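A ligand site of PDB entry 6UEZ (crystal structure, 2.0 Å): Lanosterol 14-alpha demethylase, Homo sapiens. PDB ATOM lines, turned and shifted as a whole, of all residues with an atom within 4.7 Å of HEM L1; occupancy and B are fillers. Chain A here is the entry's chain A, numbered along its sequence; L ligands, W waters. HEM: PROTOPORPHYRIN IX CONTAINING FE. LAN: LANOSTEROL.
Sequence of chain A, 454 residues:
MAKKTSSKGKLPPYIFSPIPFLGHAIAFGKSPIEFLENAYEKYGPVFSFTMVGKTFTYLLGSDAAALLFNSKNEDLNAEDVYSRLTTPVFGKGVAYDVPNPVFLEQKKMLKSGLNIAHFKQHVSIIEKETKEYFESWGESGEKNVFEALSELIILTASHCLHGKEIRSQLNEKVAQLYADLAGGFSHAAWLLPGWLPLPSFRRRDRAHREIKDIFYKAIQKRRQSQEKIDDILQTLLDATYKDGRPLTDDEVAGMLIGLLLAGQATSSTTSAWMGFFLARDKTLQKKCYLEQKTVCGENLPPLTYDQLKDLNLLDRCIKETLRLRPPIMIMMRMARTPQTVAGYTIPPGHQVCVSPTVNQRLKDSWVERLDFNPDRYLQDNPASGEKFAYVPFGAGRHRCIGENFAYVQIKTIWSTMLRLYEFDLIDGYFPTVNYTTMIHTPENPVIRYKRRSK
An iron atom (FE) of HEM L1 is bound by the side-chain sulfur of Cys 400, at 2.5 Å.
ND1 of His 398 is in hydrogen-bond range of O1D of HEM L1, at 2.5 Å.
OH of Tyr 82 lies within hydrogen-bond range of O1A of HEM L1, 2.6 Å away.
An oxygen (O1D) of HEM L1 is in hydrogen-bond range of the side-chain hydroxyl (OH) of Tyr 96, at 2.7 Å.
NH2 of Arg 333 lies within salt-bridge range of O2A of HEM L1 (2.7 Å).
O of Phe 393 sits at hydrogen-bond distance from N of Cys 400.
The backbone NH (N) of Gly 402 lies close to the side-chain sulfur (SG) of Cys 400, 3.3 Å away.
The side-chain hydroxyl (OH) of Tyr 82 sits at hydrogen-bond distance from the guanidinium group (NH1) of Arg 333, 3.3 Å away.
The backbone carbonyl oxygen of Ala 262 sits at hydrogen-bond distance from the side-chain hydroxyl of Thr 266, at 2.9 Å.
The backbone carbonyl oxygen of Thr 266 is in hydrogen-bond range of the side-chain hydroxyl of Thr 270 (2.9 Å).
Phe 103 touches HEM L1 (CE2 to CGD, 3.3 Å).
Leu 259 touches HEM L1 (CD1 to CBC, 3.9 Å).
Ala 262 touches HEM L1 (O to CMC, 3.3 Å).
Gly 263 touches HEM L1 (CA to CMC, 3.8 Å).
OG1 of Thr 266 touches CAB of HEM L1, 3.0 Å away.
Pro 327 touches HEM L1 (CG to CMB, 3.4 Å).
Ile 328 touches HEM L1 (CD1 to C4A, 3.5 Å).
Met 331 touches HEM L1 (CG to O1A, 3.3 Å).
O of Pro 392 touches CMA of HEM L1 (3.4 Å).
Phe 393 touches HEM L1 (CE1 to C3B, 3.3 Å).
N of Gly 394 touches CMA of HEM L1 (3.6 Å).
Arg 397 touches HEM L1.
Arg 399 touches HEM L1 (O to CAD, 3.7 Å).
Ile 401 touches HEM L1.
CA of Gly 402 touches C2C of HEM L1, 3.7 Å away.
CB of Ala 406 touches CBB of HEM L1, at 3.7 Å.
21 residues have an atom within 4 Å of HEM L1: Tyr 82, Tyr 96, Phe 103, Leu 259, Ala 262, Gly 263, Thr 266, Pro 327, Ile 328, Met 331, Arg 333, Pro 392, Phe 393, Gly 394, Arg 397, His 398, Arg 399, Cys 400, Ile 401, Gly 402 and Ala 406.
Water W1 lies within hydrogen-bond range of O of Arg 399 (2.6 Å), O2D of HEM L1 (2.8 Å) and O of Arg 397 (3.1 Å).
Water W3 lies within hydrogen-bond range of the backbone carbonyl oxygen of Arg 397 (3.0 Å), a ring nitrogen (ND1) of His 398 (3.1 Å) and an oxygen (O2D) of HEM L1 (3.1 Å).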
ATOM      1  N   TYR A  82      22.337  -5.255 -29.335  1.00  0.00           N
ATOM      2  CA  TYR A  82      23.076  -4.365 -28.392  1.00  0.00           C
ATOM      3  C   TYR A  82      24.247  -3.657 -29.087  1.00  0.00           C
ATOM      4  O   TYR A  82      24.568  -2.530 -28.648  1.00  0.00           O
ATOM      5  CB  TYR A  82      23.547  -5.131 -27.154  1.00  0.00           C
ATOM      6  CG  TYR A  82      22.452  -5.570 -26.215  1.00  0.00           C
ATOM      7  CD1 TYR A  82      21.213  -4.948 -26.214  1.00  0.00           C
ATOM      8  CD2 TYR A  82      22.725  -6.472 -25.199  1.00  0.00           C
ATOM      9  CE1 TYR A  82      20.229  -5.290 -25.290  1.00  0.00           C
ATOM     10  CE2 TYR A  82      21.772  -6.792 -24.237  1.00  0.00           C
ATOM     11  CZ  TYR A  82      20.519  -6.214 -24.304  1.00  0.00           C
ATOM     12  OH  TYR A  82      19.548  -6.571 -23.412  1.00  0.00           O
ATOM     13  N   TYR A  96      29.664  -6.482 -27.255  1.00  0.00           N
ATOM     14  CA  TYR A  96      28.660  -6.900 -28.270  1.00  0.00           C
ATOM     15  C   TYR A  96      29.183  -6.588 -29.675  1.00  0.00           C
ATOM     16  O   TYR A  96      28.489  -6.916 -30.663  1.00  0.00           O
ATOM     17  CB  TYR A  96      27.319  -6.254 -27.959  1.00  0.00           C
ATOM     18  CG  TYR A  96      26.784  -6.612 -26.588  1.00  0.00           C
ATOM     19  CD1 TYR A  96      26.541  -7.926 -26.250  1.00  0.00           C
ATOM     20  CD2 TYR A  96      26.617  -5.652 -25.607  1.00  0.00           C
ATOM     21  CE1 TYR A  96      26.067  -8.278 -25.000  1.00  0.00           C
ATOM     22  CE2 TYR A  96      26.137  -5.971 -24.346  1.00  0.00           C
ATOM     23  CZ  TYR A  96      25.870  -7.292 -24.042  1.00  0.00           C
ATOM     24  OH  TYR A  96      25.383  -7.633 -22.814  1.00  0.00           O
ATOM     25  N   PHE A 103      33.353 -12.707 -26.134  1.00  0.00           N
ATOM     26  CA  PHE A 103      32.830 -11.890 -25.003  1.00  0.00           C
ATOM     27  C   PHE A 103      32.847 -12.731 -23.720  1.00  0.00           C
ATOM     28  O   PHE A 103      33.219 -12.187 -22.671  1.00  0.00           O
ATOM     29  CB  PHE A 103      31.453 -11.334 -25.357  1.00  0.00           C
ATOM     30  CG  PHE A 103      30.773 -10.604 -24.234  1.00  0.00           C
ATOM     31  CD1 PHE A 103      31.449  -9.672 -23.465  1.00  0.00           C
ATOM     32  CD2 PHE A 103      29.446 -10.865 -23.935  1.00  0.00           C
ATOM     33  CE1 PHE A 103      30.814  -9.010 -22.421  1.00  0.00           C
ATOM     34  CE2 PHE A 103      28.811 -10.203 -22.890  1.00  0.00           C
ATOM     35  CZ  PHE A 103      29.500  -9.272 -22.147  1.00  0.00           C
ATOM     36  N   LYS A 107      34.320 -11.446 -20.186  1.00  0.00           N
ATOM     37  CA  LYS A 107      33.455 -11.426 -18.978  1.00  0.00           C
ATOM     38  C   LYS A 107      34.195 -12.152 -17.847  1.00  0.00           C
ATOM     39  O   LYS A 107      34.337 -11.569 -16.753  1.00  0.00           O
ATOM     40  CB  LYS A 107      32.101 -12.059 -19.342  1.00  0.00           C
ATOM     41  CG  LYS A 107      31.047 -12.089 -18.246  1.00  0.00           C
ATOM     42  CD  LYS A 107      29.743 -12.732 -18.688  1.00  0.00           C
ATOM     43  CE  LYS A 107      29.857 -14.224 -18.946  1.00  0.00           C
ATOM     44  NZ  LYS A 107      30.167 -15.018 -17.737  1.00  0.00           N
ATOM     45  N   LEU A 114      36.255  -9.968  -8.626  1.00  0.00           N
ATOM     46  CA  LEU A 114      34.941  -9.947  -7.925  1.00  0.00           C
ATOM     47  C   LEU A 114      34.854 -11.116  -6.945  1.00  0.00           C
ATOM     48  O   LEU A 114      34.172 -12.117  -7.265  1.00  0.00           O
ATOM     49  CB  LEU A 114      33.821  -9.987  -8.968  1.00  0.00           C
ATOM     50  CG  LEU A 114      33.854  -8.864 -10.003  1.00  0.00           C
ATOM     51  CD1 LEU A 114      32.702  -9.013 -10.985  1.00  0.00           C
ATOM     52  CD2 LEU A 114      33.829  -7.494  -9.350  1.00  0.00           C
ATOM     53  N   LEU A 161      37.212  -1.354  -8.460  1.00  0.00           N
ATOM     54  CA  LEU A 161      37.289  -2.275  -9.628  1.00  0.00           C
ATOM     55  C   LEU A 161      38.596  -2.040 -10.400  1.00  0.00           C
ATOM     56  O   LEU A 161      39.160  -3.037 -10.889  1.00  0.00           O
ATOM     57  CB  LEU A 161      36.072  -2.079 -10.540  1.00  0.00           C
ATOM     58  CG  LEU A 161      34.699  -2.273  -9.897  1.00  0.00           C
ATOM     59  CD1 LEU A 161      33.589  -1.939 -10.881  1.00  0.00           C
ATOM     60  CD2 LEU A 161      34.536  -3.694  -9.365  1.00  0.00           C
ATOM     61  N   LEU A 259      34.020  -1.603 -17.755  1.00  0.00           N
ATOM     62  CA  LEU A 259      33.974  -1.955 -16.314  1.00  0.00           C
ATOM     63  C   LEU A 259      33.550  -0.715 -15.525  1.00  0.00           C
ATOM     64  O   LEU A 259      32.765  -0.852 -14.593  1.00  0.00           O
ATOM     65  CB  LEU A 259      35.365  -2.421 -15.887  1.00  0.00           C
ATOM     66  CG  LEU A 259      35.457  -2.867 -14.430  1.00  0.00           C
ATOM     67  CD1 LEU A 259      34.703  -4.169 -14.229  1.00  0.00           C
ATOM     68  CD2 LEU A 259      36.904  -3.027 -14.022  1.00  0.00           C
ATOM     69  N   ALA A 262      29.784  -0.113 -16.036  1.00  0.00           N
ATOM     70  CA  ALA A 262      29.006  -1.127 -15.302  1.00  0.00           C
ATOM     71  C   ALA A 262      28.983  -0.792 -13.812  1.00  0.00           C
ATOM     72  O   ALA A 262      27.948  -1.012 -13.162  1.00  0.00           O
ATOM     73  CB  ALA A 262      29.591  -2.495 -15.528  1.00  0.00           C
ATOM     74  N   GLY A 263      30.111  -0.332 -13.282  1.00  0.00           N
ATOM     75  CA  GLY A 263      30.288   0.004 -11.853  1.00  0.00           C
ATOM     76  C   GLY A 263      29.512   1.254 -11.471  1.00  0.00           C
ATOM     77  O   GLY A 263      29.030   1.325 -10.331  1.00  0.00           O
ATOM     78  N   THR A 266      24.872   2.007 -13.425  1.00  0.00           N
ATOM     79  CA  THR A 266      23.782   1.232 -12.774  1.00  0.00           C
ATOM     80  C   THR A 266      23.580   1.662 -11.320  1.00  0.00           C
ATOM     81  O   THR A 266      22.416   1.764 -10.905  1.00  0.00           O
ATOM     82  CB  THR A 266      24.033  -0.273 -12.958  1.00  0.00           C
ATOM     83  OG1 THR A 266      25.239  -0.584 -12.266  1.00  0.00           O
ATOM     84  CG2 THR A 266      24.215  -0.646 -14.416  1.00  0.00           C
ATOM     85  N   SER A 267      24.658   1.974 -10.587  1.00  0.00           N
ATOM     86  CA  SER A 267      24.587   2.237  -9.133  1.00  0.00           C
ATOM     87  C   SER A 267      24.150   3.674  -8.824  1.00  0.00           C
ATOM     88  O   SER A 267      23.557   3.893  -7.760  1.00  0.00           O
ATOM     89  CB  SER A 267      25.898   1.933  -8.454  1.00  0.00           C
ATOM     90  OG  SER A 267      25.989   0.564  -8.085  1.00  0.00           O
ATOM     91  N   THR A 270      20.164   4.053  -9.108  1.00  0.00           N
ATOM     92  CA  THR A 270      19.605   3.232  -8.002  1.00  0.00           C
ATOM     93  C   THR A 270      19.851   3.949  -6.669  1.00  0.00           C
ATOM     94  O   THR A 270      18.895   4.075  -5.871  1.00  0.00           O
ATOM     95  CB  THR A 270      20.226   1.829  -7.981  1.00  0.00           C
ATOM     96  OG1 THR A 270      20.064   1.236  -9.265  1.00  0.00           O
ATOM     97  CG2 THR A 270      19.626   0.949  -6.908  1.00  0.00           C
ATOM     98  N   LEU A 322      15.590  -1.475  -6.382  1.00  0.00           N
ATOM     99  CA  LEU A 322      15.817  -2.215  -7.652  1.00  0.00           C
ATOM    100  C   LEU A 322      14.492  -2.812  -8.137  1.00  0.00           C
ATOM    101  O   LEU A 322      14.332  -2.839  -9.376  1.00  0.00           O
ATOM    102  CB  LEU A 322      16.882  -3.300  -7.439  1.00  0.00           C
ATOM    103  CG  LEU A 322      18.293  -2.745  -7.264  1.00  0.00           C
ATOM    104  CD1 LEU A 322      19.245  -3.797  -6.730  1.00  0.00           C
ATOM    105  CD2 LEU A 322      18.786  -2.161  -8.594  1.00  0.00           C
ATOM    106  N   PRO A 327      17.695   0.090 -13.034  1.00  0.00           N
ATOM    107  CA  PRO A 327      18.348   0.945 -14.025  1.00  0.00           C
ATOM    108  C   PRO A 327      18.238   0.394 -15.450  1.00  0.00           C
ATOM    109  O   PRO A 327      18.340   1.169 -16.389  1.00  0.00           O
ATOM    110  CB  PRO A 327      19.799   0.997 -13.531  1.00  0.00           C
ATOM    111  CG  PRO A 327      19.980  -0.274 -12.738  1.00  0.00           C
ATOM    112  CD  PRO A 327      18.642  -0.488 -12.053  1.00  0.00           C
ATOM    113  N   ILE A 328      18.109  -0.925 -15.599  1.00  0.00           N
ATOM    114  CA  ILE A 328      17.792  -1.586 -16.899  1.00  0.00           C
ATOM    115  C   ILE A 328      16.316  -1.979 -16.893  1.00  0.00           C
ATOM    116  O   ILE A 328      15.920  -2.859 -16.115  1.00  0.00           O
ATOM    117  CB  ILE A 328      18.745  -2.767 -17.160  1.00  0.00           C
ATOM    118  CG1 ILE A 328      20.155  -2.208 -17.418  1.00  0.00           C
ATOM    119  CG2 ILE A 328      18.237  -3.624 -18.307  1.00  0.00           C
ATOM    120  CD1 ILE A 328      21.276  -3.177 -17.144  1.00  0.00           C
ATOM    121  N   MET A 331      15.365  -5.698 -21.591  1.00  0.00           N
ATOM    122  CA  MET A 331      16.472  -6.471 -22.206  1.00  0.00           C
ATOM    123  C   MET A 331      15.980  -7.084 -23.514  1.00  0.00           C
ATOM    124  O   MET A 331      14.764  -7.311 -23.627  1.00  0.00           O
ATOM    125  CB  MET A 331      16.960  -7.601 -21.303  1.00  0.00           C
ATOM    126  CG  MET A 331      17.797  -7.054 -20.163  1.00  0.00           C
ATOM    127  SD  MET A 331      16.755  -6.955 -18.698  1.00  0.00           S
ATOM    128  CE  MET A 331      16.833  -8.678 -18.216  1.00  0.00           C
ATOM    129  N   ARG A 333      16.669  -9.147 -27.460  1.00  0.00           N
ATOM    130  CA  ARG A 333      17.344 -10.198 -28.263  1.00  0.00           C
ATOM    131  C   ARG A 333      16.751 -10.192 -29.681  1.00  0.00           C
ATOM    132  O   ARG A 333      15.549  -9.890 -29.828  1.00  0.00           O
ATOM    133  CB  ARG A 333      17.150 -11.576 -27.638  1.00  0.00           C
ATOM    134  CG  ARG A 333      17.509 -11.684 -26.154  1.00  0.00           C
ATOM    135  CD  ARG A 333      18.989 -11.867 -25.848  1.00  0.00           C
ATOM    136  NE  ARG A 333      19.216 -12.111 -24.429  1.00  0.00           N
ATOM    137  CZ  ARG A 333      19.403 -11.157 -23.520  1.00  0.00           C
ATOM    138  NH1 ARG A 333      19.453  -9.880 -23.864  1.00  0.00           N
ATOM    139  NH2 ARG A 333      19.588 -11.501 -22.251  1.00  0.00           N
ATOM    140  N   PRO A 392      16.262  -7.879 -11.542  1.00  0.00           N
ATOM    141  CA  PRO A 392      16.979  -6.626 -11.791  1.00  0.00           C
ATOM    142  C   PRO A 392      18.365  -6.809 -12.410  1.00  0.00           C
ATOM    143  O   PRO A 392      18.842  -5.892 -12.994  1.00  0.00           O
ATOM    144  CB  PRO A 392      17.049  -5.950 -10.422  1.00  0.00           C
ATOM    145  CG  PRO A 392      16.943  -7.074  -9.453  1.00  0.00           C
ATOM    146  CD  PRO A 392      16.081  -8.114 -10.125  1.00  0.00           C
ATOM    147  N   PHE A 393      19.004  -7.953 -12.180  1.00  0.00           N
ATOM    148  CA  PHE A 393      20.364  -8.230 -12.689  1.00  0.00           C
ATOM    149  C   PHE A 393      20.303  -9.282 -13.800  1.00  0.00           C
ATOM    150  O   PHE A 393      21.320  -9.886 -14.073  1.00  0.00           O
ATOM    151  CB  PHE A 393      21.255  -8.722 -11.535  1.00  0.00           C
ATOM    152  CG  PHE A 393      21.494  -7.704 -10.455  1.00  0.00           C
ATOM    153  CD1 PHE A 393      22.464  -6.732 -10.599  1.00  0.00           C
ATOM    154  CD2 PHE A 393      20.740  -7.706  -9.294  1.00  0.00           C
ATOM    155  CE1 PHE A 393      22.673  -5.784  -9.617  1.00  0.00           C
ATOM    156  CE2 PHE A 393      20.961  -6.764  -8.313  1.00  0.00           C
ATOM    157  CZ  PHE A 393      21.929  -5.808  -8.473  1.00  0.00           C
ATOM    158  N   GLY A 394      19.113  -9.561 -14.345  1.00  0.00           N
ATOM    159  CA  GLY A 394      18.862 -10.583 -15.376  1.00  0.00           C
ATOM    160  C   GLY A 394      18.969 -11.982 -14.801  1.00  0.00           C
ATOM    161  O   GLY A 394      19.007 -12.138 -13.557  1.00  0.00           O
ATOM    162  N   ARG A 397      22.267 -16.821 -19.507  1.00  0.00           N
ATOM    163  CA  ARG A 397      23.619 -16.798 -20.137  1.00  0.00           C
ATOM    164  C   ARG A 397      24.155 -15.363 -20.198  1.00  0.00           C
ATOM    165  O   ARG A 397      25.394 -15.205 -20.134  1.00  0.00           O
ATOM    166  CB  ARG A 397      23.530 -17.500 -21.490  1.00  0.00           C
ATOM    167  CG  ARG A 397      23.614 -19.017 -21.353  1.00  0.00           C
ATOM    168  CD  ARG A 397      23.024 -19.780 -22.521  1.00  0.00           C
ATOM    169  NE  ARG A 397      23.111 -21.225 -22.323  1.00  0.00           N
ATOM    170  CZ  ARG A 397      22.091 -22.020 -22.007  1.00  0.00           C
ATOM    171  NH1 ARG A 397      20.880 -21.529 -21.821  1.00  0.00           N
ATOM    172  NH2 ARG A 397      22.296 -23.325 -21.885  1.00  0.00           N
ATOM    173  N   HIS A 398      23.285 -14.341 -20.180  1.00  0.00           N
ATOM    174  CA  HIS A 398      23.697 -12.918 -20.223  1.00  0.00           C
ATOM    175  C   HIS A 398      23.570 -12.275 -18.837  1.00  0.00           C
ATOM    176  O   HIS A 398      23.567 -11.041 -18.772  1.00  0.00           O
ATOM    177  CB  HIS A 398      22.852 -12.134 -21.211  1.00  0.00           C
ATOM    178  CG  HIS A 398      23.151 -12.491 -22.621  1.00  0.00           C
ATOM    179  ND1 HIS A 398      24.297 -12.055 -23.252  1.00  0.00           N
ATOM    180  CD2 HIS A 398      22.531 -13.322 -23.478  1.00  0.00           C
ATOM    181  CE1 HIS A 398      24.338 -12.578 -24.457  1.00  0.00           C
ATOM    182  NE2 HIS A 398      23.271 -13.335 -24.629  1.00  0.00           N
ATOM    183  N   ARG A 399      23.506 -13.069 -17.769  1.00  0.00           N
ATOM    184  CA  ARG A 399      23.264 -12.504 -16.420  1.00  0.00           C
ATOM    185  C   ARG A 399      24.458 -11.694 -15.929  1.00  0.00           C
ATOM    186  O   ARG A 399      25.582 -11.932 -16.381  1.00  0.00           O
ATOM    187  CB  ARG A 399      22.915 -13.611 -15.427  1.00  0.00           C
ATOM    188  CG  ARG A 399      24.121 -14.395 -14.948  1.00  0.00           C
ATOM    189  CD  ARG A 399      23.675 -15.645 -14.239  1.00  0.00           C
ATOM    190  NE  ARG A 399      24.830 -16.386 -13.771  1.00  0.00           N
ATOM    191  CZ  ARG A 399      25.332 -17.425 -14.414  1.00  0.00           C
ATOM    192  NH1 ARG A 399      24.750 -17.868 -15.515  1.00  0.00           N
ATOM    193  NH2 ARG A 399      26.399 -18.044 -13.932  1.00  0.00           N
ATOM    194  N   CYS A 400      24.202 -10.791 -14.988  1.00  0.00           N
ATOM    195  CA  CYS A 400      25.198  -9.880 -14.386  1.00  0.00           C
ATOM    196  C   CYS A 400      26.274 -10.672 -13.632  1.00  0.00           C
ATOM    197  O   CYS A 400      25.940 -11.719 -13.098  1.00  0.00           O
ATOM    198  CB  CYS A 400      24.492  -9.006 -13.354  1.00  0.00           C
ATOM    199  SG  CYS A 400      25.417  -7.512 -12.924  1.00  0.00           S
ATOM    200  N   ILE A 401      27.468 -10.076 -13.516  1.00  0.00           N
ATOM    201  CA  ILE A 401      28.602 -10.594 -12.692  1.00  0.00           C
ATOM    202  C   ILE A 401      28.833  -9.645 -11.518  1.00  0.00           C
ATOM    203  O   ILE A 401      29.602 -10.019 -10.626  1.00  0.00           O
ATOM    204  CB  ILE A 401      29.875 -10.757 -13.539  1.00  0.00           C
ATOM    205  CG1 ILE A 401      30.382  -9.400 -14.051  1.00  0.00           C
ATOM    206  CG2 ILE A 401      29.668 -11.750 -14.661  1.00  0.00           C
ATOM    207  CD1 ILE A 401      31.731  -9.454 -14.718  1.00  0.00           C
ATOM    208  N   GLY A 402      28.215  -8.467 -11.512  1.00  0.00           N
ATOM    209  CA  GLY A 402      28.515  -7.458 -10.480  1.00  0.00           C
ATOM    210  C   GLY A 402      27.439  -7.284  -9.420  1.00  0.00           C
ATOM    211  O   GLY A 402      27.524  -6.284  -8.696  1.00  0.00           O
ATOM    212  N   PHE A 405      29.119  -6.926  -5.993  1.00  0.00           N
ATOM    213  CA  PHE A 405      29.878  -5.652  -5.908  1.00  0.00           C
ATOM    214  C   PHE A 405      28.885  -4.487  -5.783  1.00  0.00           C
ATOM    215  O   PHE A 405      29.136  -3.574  -4.967  1.00  0.00           O
ATOM    216  CB  PHE A 405      30.843  -5.434  -7.080  1.00  0.00           C
ATOM    217  CG  PHE A 405      31.465  -4.071  -7.041  1.00  0.00           C
ATOM    218  CD1 PHE A 405      32.391  -3.738  -6.060  1.00  0.00           C
ATOM    219  CD2 PHE A 405      30.951  -3.041  -7.810  1.00  0.00           C
ATOM    220  CE1 PHE A 405      32.895  -2.453  -5.957  1.00  0.00           C
ATOM    221  CE2 PHE A 405      31.436  -1.750  -7.693  1.00  0.00           C
ATOM    222  CZ  PHE A 405      32.421  -1.462  -6.768  1.00  0.00           C
ATOM    223  N   ALA A 406      27.812  -4.491  -6.576  1.00  0.00           N
ATOM    224  CA  ALA A 406      26.821  -3.389  -6.573  1.00  0.00           C
ATOM    225  C   ALA A 406      26.214  -3.230  -5.184  1.00  0.00           C
ATOM    226  O   ALA A 406      26.107  -2.080  -4.702  1.00  0.00           O
ATOM    227  CB  ALA A 406      25.762  -3.639  -7.623  1.00  0.00           C
ATOM    228  N   ILE A 410      26.563   0.136  -2.945  1.00  0.00           N
ATOM    229  CA  ILE A 410      25.351   0.910  -2.554  1.00  0.00           C
ATOM    230  C   ILE A 410      25.159   0.851  -1.033  1.00  0.00           C
ATOM    231  O   ILE A 410      24.754   1.892  -0.453  1.00  0.00           O
ATOM    232  CB  ILE A 410      24.114   0.395  -3.307  1.00  0.00           C
ATOM    233  CG1 ILE A 410      24.261   0.603  -4.826  1.00  0.00           C
ATOM    234  CG2 ILE A 410      22.846   1.058  -2.780  1.00  0.00           C
ATOM    235  CD1 ILE A 410      23.316  -0.239  -5.635  1.00  0.00           C
HETATM  236  CHA HEM L   1      24.452  -7.909 -17.340  1.00  0.00           C
HETATM  237  CHB HEM L   1      21.928  -5.174 -14.273  1.00  0.00           C
HETATM  238  CHC HEM L   1      26.078  -3.754 -12.133  1.00  0.00           C
HETATM  239  CHD HEM L   1      28.553  -6.397 -15.330  1.00  0.00           C
HETATM  240  C1A HEM L   1      23.432  -7.257 -16.685  1.00  0.00           C
HETATM  241  C2A HEM L   1      22.093  -7.450 -17.039  1.00  0.00           C
HETATM  242  C3A HEM L   1      21.398  -6.659 -16.179  1.00  0.00           C
HETATM  243  C4A HEM L   1      22.292  -6.013 -15.315  1.00  0.00           C
HETATM  244  CMA HEM L   1      19.909  -6.528 -16.142  1.00  0.00           C
HETATM  245  CAA HEM L   1      21.496  -8.370 -18.070  1.00  0.00           C
HETATM  246  CBA HEM L   1      21.517  -7.815 -19.501  1.00  0.00           C
HETATM  247  CGA HEM L   1      20.732  -8.620 -20.517  1.00  0.00           C
HETATM  248  O1A HEM L   1      20.538  -8.196 -21.668  1.00  0.00           O
HETATM  249  O2A HEM L   1      20.295  -9.764 -20.249  1.00  0.00           O
HETATM  250  C1B HEM L   1      22.860  -4.592 -13.419  1.00  0.00           C
HETATM  251  C2B HEM L   1      22.488  -3.767 -12.326  1.00  0.00           C
HETATM  252  C3B HEM L   1      23.635  -3.380 -11.720  1.00  0.00           C
HETATM  253  C4B HEM L   1      24.751  -3.974 -12.481  1.00  0.00           C
HETATM  254  CMB HEM L   1      21.113  -3.360 -11.893  1.00  0.00           C
HETATM  255  CAB HEM L   1      23.801  -2.514 -10.550  1.00  0.00           C
HETATM  256  CBB HEM L   1      22.882  -2.446  -9.598  1.00  0.00           C
HETATM  257  C1C HEM L   1      27.121  -4.351 -12.827  1.00  0.00           C
HETATM  258  C2C HEM L   1      28.461  -4.299 -12.465  1.00  0.00           C
HETATM  259  C3C HEM L   1      29.163  -5.048 -13.387  1.00  0.00           C
HETATM  260  C4C HEM L   1      28.222  -5.589 -14.287  1.00  0.00           C
HETATM  261  CMC HEM L   1      28.983  -3.538 -11.276  1.00  0.00           C
HETATM  262  CAC HEM L   1      30.591  -5.369 -13.469  1.00  0.00           C
HETATM  263  CBC HEM L   1      31.400  -5.204 -12.434  1.00  0.00           C
HETATM  264  C1D HEM L   1      27.565  -6.996 -16.117  1.00  0.00           C
HETATM  265  C2D HEM L   1      27.959  -7.914 -17.171  1.00  0.00           C
HETATM  266  C3D HEM L   1      26.834  -8.322 -17.766  1.00  0.00           C
HETATM  267  C4D HEM L   1      25.770  -7.654 -17.015  1.00  0.00           C
HETATM  268  CMD HEM L   1      29.362  -8.295 -17.544  1.00  0.00           C
HETATM  269  CAD HEM L   1      26.770  -9.414 -18.805  1.00  0.00           C
HETATM  270  CBD HEM L   1      26.266  -9.043 -20.198  1.00  0.00           C
HETATM  271  CGD HEM L   1      26.113 -10.284 -21.022  1.00  0.00           C
HETATM  272  O1D HEM L   1      25.598 -10.220 -22.154  1.00  0.00           O
HETATM  273  O2D HEM L   1      26.499 -11.403 -20.625  1.00  0.00           O
HETATM  274  NA  HEM L   1      23.553  -6.392 -15.623  1.00  0.00           N
HETATM  275  NB  HEM L   1      24.190  -4.708 -13.447  1.00  0.00           N
HETATM  276  NC  HEM L   1      26.996  -5.156 -13.910  1.00  0.00           N
HETATM  277  ND  HEM L   1      26.234  -6.879 -16.034  1.00  0.00           N
HETATM  278 FE   HEM L   1      25.266  -5.901 -14.772  1.00  0.00          FE
HETATM  279  C6  LAN L   2      24.202  -2.332 -20.118  1.00  0.00           C
HETATM  280  C5  LAN L   2      23.967  -0.862 -20.193  1.00  0.00           C
HETATM  281  C4  LAN L   2      22.939  -0.417 -21.221  1.00  0.00           C
HETATM  282  C3  LAN L   2      21.787  -1.413 -21.234  1.00  0.00           C
HETATM  283  C25 LAN L   2      20.464  -0.878 -21.852  1.00  0.00           C
HETATM  284  C26 LAN L   2      20.610  -0.612 -23.358  1.00  0.00           C
HETATM  285  C27 LAN L   2      19.933   0.424 -21.220  1.00  0.00           C
HETATM  286  C28 LAN L   2      19.435  -1.988 -21.627  1.00  0.00           C
HETATM  287  O29 LAN L   2      18.136  -1.627 -22.099  1.00  0.00           O
HETATM  288  C30 LAN L   2      19.849  -3.307 -22.229  1.00  0.00           C
HETATM  289  C31 LAN L   2      21.142  -3.814 -21.580  1.00  0.00           C
HETATM  290  C1  LAN L   2      22.306  -2.810 -21.694  1.00  0.00           C
HETATM  291  C2  LAN L   2      22.850  -2.844 -23.144  1.00  0.00           C
HETATM  292  C24 LAN L   2      23.460  -3.232 -20.779  1.00  0.00           C
HETATM  293  C23 LAN L   2      23.834  -4.700 -20.748  1.00  0.00           C
HETATM  294  C22 LAN L   2      25.254  -5.109 -20.318  1.00  0.00           C
HETATM  295  C10 LAN L   2      26.178  -3.903 -20.157  1.00  0.00           C
HETATM  296  C11 LAN L   2      26.532  -3.347 -21.546  1.00  0.00           C
HETATM  297  C7  LAN L   2      25.394  -2.822 -19.322  1.00  0.00           C
HETATM  298  C8  LAN L   2      24.828  -3.393 -17.997  1.00  0.00           C
HETATM  299  C9  LAN L   2      26.487  -1.819 -18.961  1.00  0.00           C
HETATM  300  C21 LAN L   2      27.729  -2.701 -18.712  1.00  0.00           C
HETATM  301  C12 LAN L   2      27.470  -4.110 -19.320  1.00  0.00           C
HETATM  302  C13 LAN L   2      28.751  -4.666 -19.979  1.00  0.00           C
HETATM  303  C20 LAN L   2      28.551  -6.052 -20.591  1.00  0.00           C
HETATM  304  C14 LAN L   2      29.912  -4.665 -18.978  1.00  0.00           C
HETATM  305  C15 LAN L   2      31.248  -5.190 -19.510  1.00  0.00           C
HETATM  306  C16 LAN L   2      31.816  -4.337 -20.597  1.00  0.00           C
HETATM  307  C17 LAN L   2      32.860  -4.579 -21.379  1.00  0.00           C
HETATM  308  C19 LAN L   2      33.347  -3.614 -22.416  1.00  0.00           C
HETATM  309  C18 LAN L   2      33.603  -5.883 -21.342  1.00  0.00           C
HETATM  310  O   HOH W   1      26.825 -13.069 -18.344  1.00  0.00           O
HETATM  311  O   HOH W   2      19.960 -11.740 -18.351  1.00  0.00           O
HETATM  312  O   HOH W   3      26.617 -13.901 -22.507  1.00  0.00           O
